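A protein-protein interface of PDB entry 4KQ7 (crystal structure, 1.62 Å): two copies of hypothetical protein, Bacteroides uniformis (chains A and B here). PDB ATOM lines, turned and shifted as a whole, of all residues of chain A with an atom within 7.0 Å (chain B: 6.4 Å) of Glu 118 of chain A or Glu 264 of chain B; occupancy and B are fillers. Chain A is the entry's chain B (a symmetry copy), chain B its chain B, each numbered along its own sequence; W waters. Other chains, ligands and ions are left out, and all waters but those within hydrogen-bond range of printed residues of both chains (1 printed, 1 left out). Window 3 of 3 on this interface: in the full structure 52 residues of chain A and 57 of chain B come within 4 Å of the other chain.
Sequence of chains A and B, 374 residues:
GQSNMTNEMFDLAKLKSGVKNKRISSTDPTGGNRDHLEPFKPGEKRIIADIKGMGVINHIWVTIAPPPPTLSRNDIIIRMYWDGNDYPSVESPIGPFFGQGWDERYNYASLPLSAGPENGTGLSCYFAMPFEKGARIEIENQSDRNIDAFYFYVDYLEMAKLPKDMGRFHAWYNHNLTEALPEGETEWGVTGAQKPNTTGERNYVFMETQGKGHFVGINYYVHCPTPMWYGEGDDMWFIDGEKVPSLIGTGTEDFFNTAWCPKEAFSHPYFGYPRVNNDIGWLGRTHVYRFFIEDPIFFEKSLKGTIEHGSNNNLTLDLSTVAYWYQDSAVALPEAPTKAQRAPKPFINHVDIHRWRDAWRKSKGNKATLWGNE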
ATOM      1  N   PRO A  67      -2.951   0.241  11.697  1.00  0.00           N
ATOM      2  CA  PRO A  67      -2.818   1.619  11.201  1.00  0.00           C
ATOM      3  C   PRO A  67      -1.422   2.188  11.489  1.00  0.00           C
ATOM      4  O   PRO A  67      -0.650   1.554  12.210  1.00  0.00           O
ATOM      5  CB  PRO A  67      -3.902   2.372  12.003  1.00  0.00           C
ATOM      6  CG  PRO A  67      -4.053   1.607  13.277  1.00  0.00           C
ATOM      7  CD  PRO A  67      -3.552   0.201  13.053  1.00  0.00           C
ATOM      8  N   ARG A  73       2.533   3.539   6.056  1.00  0.00           N
ATOM      9  CA  ARG A  73       2.040   3.474   4.673  1.00  0.00           C
ATOM     10  C   ARG A  73       3.093   4.017   3.696  1.00  0.00           C
ATOM     11  O   ARG A  73       2.878   4.008   2.481  1.00  0.00           O
ATOM     12  CB  ARG A  73       0.701   4.185   4.533  1.00  0.00           C
ATOM     13  CG  ARG A  73      -0.347   3.511   5.439  1.00  0.00           C
ATOM     14  CD  ARG A  73      -1.628   4.312   5.500  1.00  0.00           C
ATOM     15  NE  ARG A  73      -1.438   5.605   6.169  1.00  0.00           N
ATOM     16  CZ  ARG A  73      -2.421   6.480   6.351  1.00  0.00           C
ATOM     17  NH1 ARG A  73      -3.647   6.211   5.920  1.00  0.00           N
ATOM     18  NH2 ARG A  73      -2.186   7.634   6.961  1.00  0.00           N
ATOM     19  N   ARG A 105      -0.445  10.149   9.869  1.00  0.00           N
ATOM     20  CA  ARG A 105      -1.870  10.036   9.556  1.00  0.00           C
ATOM     21  C   ARG A 105      -2.551  11.338   9.961  1.00  0.00           C
ATOM     22  O   ARG A 105      -2.240  11.906  11.017  1.00  0.00           O
ATOM     23  CB  ARG A 105      -2.499   8.810  10.266  1.00  0.00           C
ATOM     24  CG  ARG A 105      -2.435   8.875  11.806  1.00  0.00           C
ATOM     25  CD  ARG A 105      -2.879   7.565  12.441  1.00  0.00           C
ATOM     26  NE  ARG A 105      -4.321   7.333  12.268  1.00  0.00           N
ATOM     27  CZ  ARG A 105      -4.999   6.381  12.899  1.00  0.00           C
ATOM     28  NH1 ARG A 105      -4.373   5.538  13.714  1.00  0.00           N
ATOM     29  NH2 ARG A 105      -6.310   6.257  12.711  1.00  0.00           N
ATOM     30  N   TYR A 106      -3.422  11.847   9.088  1.00  0.00           N
ATOM     31  CA  TYR A 106      -4.159  13.089   9.359  1.00  0.00           C
ATOM     32  C   TYR A 106      -5.287  13.225   8.368  1.00  0.00           C
ATOM     33  O   TYR A 106      -5.128  12.921   7.180  1.00  0.00           O
ATOM     34  CB  TYR A 106      -3.253  14.357   9.324  1.00  0.00           C
ATOM     35  CG  TYR A 106      -2.251  14.379   8.182  1.00  0.00           C
ATOM     36  CD1 TYR A 106      -2.577  14.942   6.950  1.00  0.00           C
ATOM     37  CD2 TYR A 106      -0.974  13.843   8.339  1.00  0.00           C
ATOM     38  CE1 TYR A 106      -1.678  14.914   5.881  1.00  0.00           C
ATOM     39  CE2 TYR A 106      -0.056  13.832   7.282  1.00  0.00           C
ATOM     40  CZ  TYR A 106      -0.415  14.369   6.055  1.00  0.00           C
ATOM     41  OH  TYR A 106       0.494  14.355   5.020  1.00  0.00           O
ATOM     42  N   ASN A 107      -6.447  13.686   8.856  1.00  0.00           N
ATOM     43  CA  ASN A 107      -7.575  13.885   7.945  1.00  0.00           C
ATOM     44  C   ASN A 107      -7.359  15.067   7.026  1.00  0.00           C
ATOM     45  O   ASN A 107      -6.905  16.116   7.482  1.00  0.00           O
ATOM     46  CB  ASN A 107      -8.866  14.172   8.741  1.00  0.00           C
ATOM     47  CG  ASN A 107      -9.408  13.014   9.529  1.00  0.00           C
ATOM     48  OD1 ASN A 107      -9.297  11.861   9.128  1.00  0.00           O
ATOM     49  ND2 ASN A 107     -10.070  13.312  10.663  1.00  0.00           N
ATOM     50  N   GLY A 116      -9.605  10.286   4.882  1.00  0.00           N
ATOM     51  CA  GLY A 116     -10.671  10.598   5.822  1.00  0.00           C
ATOM     52  C   GLY A 116     -10.602   9.806   7.100  1.00  0.00           C
ATOM     53  O   GLY A 116      -9.697   9.000   7.309  1.00  0.00           O
ATOM     54  N   PRO A 117     -11.590  10.021   7.970  1.00  0.00           N
ATOM     55  CA  PRO A 117     -11.627   9.317   9.260  1.00  0.00           C
ATOM     56  C   PRO A 117     -11.608   7.782   9.116  1.00  0.00           C
ATOM     57  O   PRO A 117     -12.023   7.293   8.075  1.00  0.00           O
ATOM     58  CB  PRO A 117     -12.960   9.781   9.857  1.00  0.00           C
ATOM     59  CG  PRO A 117     -13.171  11.145   9.301  1.00  0.00           C
ATOM     60  CD  PRO A 117     -12.701  10.988   7.855  1.00  0.00           C
ATOM     61  N   GLU A 118     -11.094   7.019  10.106  1.00  0.00           N
ATOM     62  CA  GLU A 118     -10.582   7.465  11.407  1.00  0.00           C
ATOM     63  C   GLU A 118      -9.169   8.046  11.277  1.00  0.00           C
ATOM     64  O   GLU A 118      -8.256   7.331  10.861  1.00  0.00           O
ATOM     65  CB  GLU A 118     -10.580   6.274  12.393  1.00  0.00           C
ATOM     66  CG  GLU A 118      -9.922   6.531  13.747  1.00  0.00           C
ATOM     67  CD  GLU A 118     -10.529   7.592  14.646  1.00  0.00           C
ATOM     68  OE1 GLU A 118     -11.700   7.968  14.414  1.00  0.00           O
ATOM     69  OE2 GLU A 118      -9.837   8.042  15.590  1.00  0.00           O
ATOM     70  N   ASN A 119      -9.010   9.347  11.619  1.00  0.00           N
ATOM     71  CA  ASN A 119      -7.735  10.082  11.587  1.00  0.00           C
ATOM     72  C   ASN A 119      -6.817   9.676  10.399  1.00  0.00           C
ATOM     73  O   ASN A 119      -5.757   9.077  10.594  1.00  0.00           O
ATOM     74  CB  ASN A 119      -6.994   9.925  12.928  1.00  0.00           C
ATOM     75  CG  ASN A 119      -5.790  10.829  13.078  1.00  0.00           C
ATOM     76  OD1 ASN A 119      -5.671  11.858  12.410  1.00  0.00           O
ATOM     77  ND2 ASN A 119      -4.888  10.451  13.962  1.00  0.00           N
ATOM     78  N   GLY A 120      -7.304   9.931   9.197  1.00  0.00           N
ATOM     79  CA  GLY A 120      -6.564   9.735   7.948  1.00  0.00           C
ATOM     80  C   GLY A 120      -6.419   8.321   7.414  1.00  0.00           C
ATOM     81  O   GLY A 120      -5.636   8.117   6.473  1.00  0.00           O
ATOM     82  N   THR A 121      -7.181   7.344   7.959  1.00  0.00           N
ATOM     83  CA  THR A 121      -7.036   5.956   7.480  1.00  0.00           C
ATOM     84  C   THR A 121      -7.926   5.601   6.281  1.00  0.00           C
ATOM     85  O   THR A 121      -7.647   4.601   5.624  1.00  0.00           O
ATOM     86  CB  THR A 121      -7.276   4.933   8.605  1.00  0.00           C
ATOM     87  OG1 THR A 121      -8.564   5.144   9.205  1.00  0.00           O
ATOM     88  CG2 THR A 121      -6.156   4.945   9.628  1.00  0.00           C
ATOM     89  N   GLY A 122      -8.959   6.396   5.984  1.00  0.00           N
ATOM     90  CA  GLY A 122      -9.824   6.113   4.829  1.00  0.00           C
ATOM     91  C   GLY A 122      -9.294   6.779   3.578  1.00  0.00           C
ATOM     92  O   GLY A 122      -9.463   7.985   3.425  1.00  0.00           O
ATOM     93  N   THR B 258     -14.491   6.069   4.219  1.00  0.00           N
ATOM     94  CA  THR B 258     -13.823   6.220   5.511  1.00  0.00           C
ATOM     95  C   THR B 258     -13.396   4.833   5.983  1.00  0.00           C
ATOM     96  O   THR B 258     -13.473   3.867   5.211  1.00  0.00           O
ATOM     97  CB  THR B 258     -14.718   7.013   6.477  1.00  0.00           C
ATOM     98  OG1 THR B 258     -16.034   6.412   6.531  1.00  0.00           O
ATOM     99  CG2 THR B 258     -14.841   8.475   6.042  1.00  0.00           C
ATOM    100  N   ALA B 259     -12.879   4.728   7.212  1.00  0.00           N
ATOM    101  CA  ALA B 259     -12.308   3.465   7.662  1.00  0.00           C
ATOM    102  C   ALA B 259     -12.213   3.367   9.159  1.00  0.00           C
ATOM    103  O   ALA B 259     -12.195   4.394   9.849  1.00  0.00           O
ATOM    104  CB  ALA B 259     -10.894   3.325   7.099  1.00  0.00           C
ATOM    105  N   TRP B 260     -12.067   2.131   9.661  1.00  0.00           N
ATOM    106  CA  TRP B 260     -11.747   1.906  11.073  1.00  0.00           C
ATOM    107  C   TRP B 260     -12.812   2.451  12.050  1.00  0.00           C
ATOM    108  O   TRP B 260     -12.450   3.078  13.043  1.00  0.00           O
ATOM    109  CB  TRP B 260     -10.362   2.545  11.375  1.00  0.00           C
ATOM    110  CG  TRP B 260      -9.215   1.638  11.057  1.00  0.00           C
ATOM    111  CD1 TRP B 260      -8.517   1.551   9.880  1.00  0.00           C
ATOM    112  CD2 TRP B 260      -8.573   0.749  11.981  1.00  0.00           C
ATOM    113  NE1 TRP B 260      -7.500   0.620  10.006  1.00  0.00           N
ATOM    114  CE2 TRP B 260      -7.524   0.105  11.286  1.00  0.00           C
ATOM    115  CE3 TRP B 260      -8.802   0.419  13.332  1.00  0.00           C
ATOM    116  CZ2 TRP B 260      -6.721  -0.877  11.891  1.00  0.00           C
ATOM    117  CZ3 TRP B 260      -8.008  -0.555  13.928  1.00  0.00           C
ATOM    118  CH2 TRP B 260      -6.984  -1.193  13.210  1.00  0.00           C
ATOM    119  N   CYS B 261     -14.117   2.184  11.779  1.00  0.00           N
ATOM    120  CA  CYS B 261     -15.221   2.521  12.697  1.00  0.00           C
ATOM    121  C   CYS B 261     -15.118   3.993  13.160  1.00  0.00           C
ATOM    122  O   CYS B 261     -14.999   4.258  14.358  1.00  0.00           O
ATOM    123  CB  CYS B 261     -15.193   1.571  13.889  1.00  0.00           C
ATOM    124  SG  CYS B 261     -14.864  -0.157  13.448  1.00  0.00           S
ATOM    125  N   PRO B 262     -15.105   4.962  12.225  1.00  0.00           N
ATOM    126  CA  PRO B 262     -14.905   6.357  12.637  1.00  0.00           C
ATOM    127  C   PRO B 262     -16.135   6.976  13.255  1.00  0.00           C
ATOM    128  O   PRO B 262     -17.235   6.489  13.025  1.00  0.00           O
ATOM    129  CB  PRO B 262     -14.604   7.061  11.313  1.00  0.00           C
ATOM    130  CG  PRO B 262     -15.441   6.286  10.291  1.00  0.00           C
ATOM    131  CD  PRO B 262     -15.298   4.851  10.761  1.00  0.00           C
ATOM    132  N   LYS B 263     -15.944   8.088  13.971  1.00  0.00           N
ATOM    133  CA  LYS B 263     -17.064   8.852  14.530  1.00  0.00           C
ATOM    134  C   LYS B 263     -16.611  10.293  14.679  1.00  0.00           C
ATOM    135  O   LYS B 263     -16.838  10.931  15.714  1.00  0.00           O
ATOM    136  CB  LYS B 263     -17.621   8.248  15.833  1.00  0.00           C
ATOM    137  CG  LYS B 263     -16.564   7.922  16.896  1.00  0.00           C
ATOM    138  CD  LYS B 263     -17.300   7.519  18.165  1.00  0.00           C
ATOM    139  CE  LYS B 263     -16.388   7.228  19.324  1.00  0.00           C
ATOM    140  NZ  LYS B 263     -17.165   7.181  20.602  1.00  0.00           N
ATOM    141  N   GLU B 264     -15.970  10.806  13.608  1.00  0.00           N
ATOM    142  CA  GLU B 264     -15.428  12.162  13.518  1.00  0.00           C
ATOM    143  C   GLU B 264     -16.150  12.949  12.435  1.00  0.00           C
ATOM    144  O   GLU B 264     -16.345  12.418  11.339  1.00  0.00           O
ATOM    145  CB  GLU B 264     -13.908  12.130  13.169  1.00  0.00           C
ATOM    146  CG  GLU B 264     -13.043  11.185  13.989  1.00  0.00           C
ATOM    147  CD  GLU B 264     -11.573  11.104  13.609  1.00  0.00           C
ATOM    148  OE1 GLU B 264     -11.259  11.073  12.397  1.00  0.00           O
ATOM    149  OE2 GLU B 264     -10.734  11.010  14.534  1.00  0.00           O
ATOM    150  N   ALA B 265     -16.480  14.232  12.701  1.00  0.00           N
ATOM    151  CA  ALA B 265     -17.077  15.096  11.662  1.00  0.00           C
ATOM    152  C   ALA B 265     -16.043  15.288  10.538  1.00  0.00           C
ATOM    153  O   ALA B 265     -14.830  15.323  10.801  1.00  0.00           O
ATOM    154  CB  ALA B 265     -17.495  16.437  12.238  1.00  0.00           C
ATOM    155  N   PHE B 266     -16.501  15.232   9.285  1.00  0.00           N
ATOM    156  CA  PHE B 266     -15.619  15.324   8.124  1.00  0.00           C
ATOM    157  C   PHE B 266     -16.410  15.801   6.939  1.00  0.00           C
ATOM    158  O   PHE B 266     -17.584  15.421   6.774  1.00  0.00           O
ATOM    159  CB  PHE B 266     -14.965  13.969   7.813  1.00  0.00           C
ATOM    160  CG  PHE B 266     -13.927  14.005   6.718  1.00  0.00           C
ATOM    161  CD1 PHE B 266     -12.641  14.484   6.968  1.00  0.00           C
ATOM    162  CD2 PHE B 266     -14.217  13.519   5.447  1.00  0.00           C
ATOM    163  CE1 PHE B 266     -11.667  14.483   5.960  1.00  0.00           C
ATOM    164  CE2 PHE B 266     -13.252  13.545   4.430  1.00  0.00           C
ATOM    165  CZ  PHE B 266     -11.973  14.009   4.705  1.00  0.00           C
ATOM    166  N   TYR B 273     -19.453  13.214   7.065  1.00  0.00           N
ATOM    167  CA  TYR B 273     -20.145  12.915   8.315  1.00  0.00           C
ATOM    168  C   TYR B 273     -20.546  14.241   8.952  1.00  0.00           C
ATOM    169  O   TYR B 273     -19.783  14.776   9.755  1.00  0.00           O
ATOM    170  CB  TYR B 273     -19.224  12.145   9.283  1.00  0.00           C
ATOM    171  CG  TYR B 273     -18.995  10.692   8.943  1.00  0.00           C
ATOM    172  CD1 TYR B 273     -18.185  10.323   7.866  1.00  0.00           C
ATOM    173  CD2 TYR B 273     -19.519   9.679   9.742  1.00  0.00           C
ATOM    174  CE1 TYR B 273     -17.926   8.986   7.584  1.00  0.00           C
ATOM    175  CE2 TYR B 273     -19.240   8.339   9.486  1.00  0.00           C
ATOM    176  CZ  TYR B 273     -18.459   7.995   8.394  1.00  0.00           C
ATOM    177  OH  TYR B 273     -18.186   6.667   8.145  1.00  0.00           O
ATOM    178  N   VAL B 276     -22.228  13.318  14.128  1.00  0.00           N
ATOM    179  CA  VAL B 276     -21.651  12.084  14.679  1.00  0.00           C
ATOM    180  C   VAL B 276     -22.246  11.829  16.063  1.00  0.00           C
ATOM    181  O   VAL B 276     -22.888  12.718  16.631  1.00  0.00           O
ATOM    182  CB  VAL B 276     -20.092  12.072  14.655  1.00  0.00           C
ATOM    183  CG1 VAL B 276     -19.584  11.973  13.212  1.00  0.00           C
ATOM    184  CG2 VAL B 276     -19.507  13.297  15.351  1.00  0.00           C
HETATM  185  O   HOH W   1      -8.474  13.072  13.969  1.00  0.00           O
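The side-chain carboxylate (OE1) of Glu 264 of chain B lies within hydrogen-bond range of the side-chain amide nitrogen (ND2) of Asn 107 of chain A (3.1 Å). The side-chain carboxylate (OE1) of Glu 264 of chain B sits at hydrogen-bond distance from the backbone NH (N) of Asn 119 of chain A. N of Ala 259 of chain B sits at hydrogen-bond distance from O of Pro 117 of chain A. The side-chain carboxylate of Glu 264 of chain B sits close to the side-chain carboxylate of Glu 118 of chain A. The backbone carbonyl oxygen of Ala 259 of chain B sits at hydrogen-bond distance from the backbone NH of Glu 118 of chain A, at 2.9 Å.
The backbone carbonyl oxygen of Glu 118 of chain A lies within hydrogen-bond range of the side-chain hydroxyl of Thr 121 of chain A. O of Gly 116 of chain A sits close to OD1 of Asn 107 of chain A (3.4 Å). The backbone NH (N) of Gly 116 of chain A lies within hydrogen-bond range of the backbone carbonyl oxygen (O) of Gly 122 of chain A (2.7 Å). The backbone carbonyl oxygen of Gly 116 of chain A lies within hydrogen-bond range of the backbone NH of Thr 121 of chain A (3.1 Å). The guanidinium group of Arg 105 of chain A sits at hydrogen-bond distance from the backbone carbonyl oxygen of Glu 118 of chain A (2.9 Å). The side-chain amide oxygen (OD1) of Asn 107 of chain A lies within hydrogen-bond range of the backbone NH (N) of Gly 120 of chain A (2.8 Å).
Arg 105 of chain A touches none of the printed residues of chain B. Tyr 106 of chain A touches none of the printed residues of chain B. Of the printed residues of chain B, Gly 116 of chain A touches Phe 266 (3.8 Å). Printed residues of chain A within 4 Å of Pro 262 of chain B: Pro 117 and Glu 118. Printed residues of chain A within 4 Å of Glu 264 of chain B: Asn 107, Pro 117, Glu 118 and Asn 119. Of the printed residues of chain A, Phe 266 of chain B touches Asn 107, Gly 116 and Pro 117. The nearest printed residue of chain A that does not touch Phe 266 of chain B is Gly 122 of chain A (6.7 Å).
No position is printed for both chains. Of the 18 pairs that touch across the chains among the printed residues, none has its exchanged pair printed and touching as well.
Printed residues of chain A that touch a printed residue of chain B: Pro 67, Asn 107, Gly 116, Pro 117, Glu 118, Asn 119, Thr 121 and Gly 122. Hydrophobic or aromatic side chains of chain A within 4 Å of the printed part of chain B: Pro 67 and Pro 117. Of the 11 printed residues of chain B, 6 touch a printed residue of chain A. Printed residues of chain B that touch a printed residue of chain A: Thr 258, Ala 259, Trp 260, Pro 262, Glu 264 and Phe 266.
Among the printed residues, merely in contact across the chains: Pro 117 of chain A with Thr 258 of chain B (3.1 Å), Pro 117 of chain A with Glu 264 of chain B (3.3 Å), Pro 117 of chain A with Phe 266 of chain B (3.4 Å), Pro 117 of chain A with Pro 262 of chain B (3.5 Å), Pro 67 of chain A with Trp 260 of chain B (3.5 Å), Thr 121 of chain A with Ala 259 of chain B (3.6 Å), Thr 121 of chain A with Trp 260 of chain B (3.7 Å), Glu 118 of chain A with Pro 262 of chain B (3.7 Å), Gly 122 of chain A with Ala 259 of chain B (3.8 Å), Glu 118 of chain A with Trp 260 of chain B (3.8 Å), Gly 116 of chain A with Phe 266 of chain B (3.8 Å), Asn 107 of chain A with Phe 266 of chain B (3.96 Å) and Gly 122 of chain A with Thr 258 of chain B (3.97 Å).
Water W1 lies within hydrogen-bond range of the side-chain carboxylate (OE2) of Glu 264 of chain B (3.1 Å) and the side-chain amide oxygen (OD1) of Asn 119 of chain A (3.4 Å).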
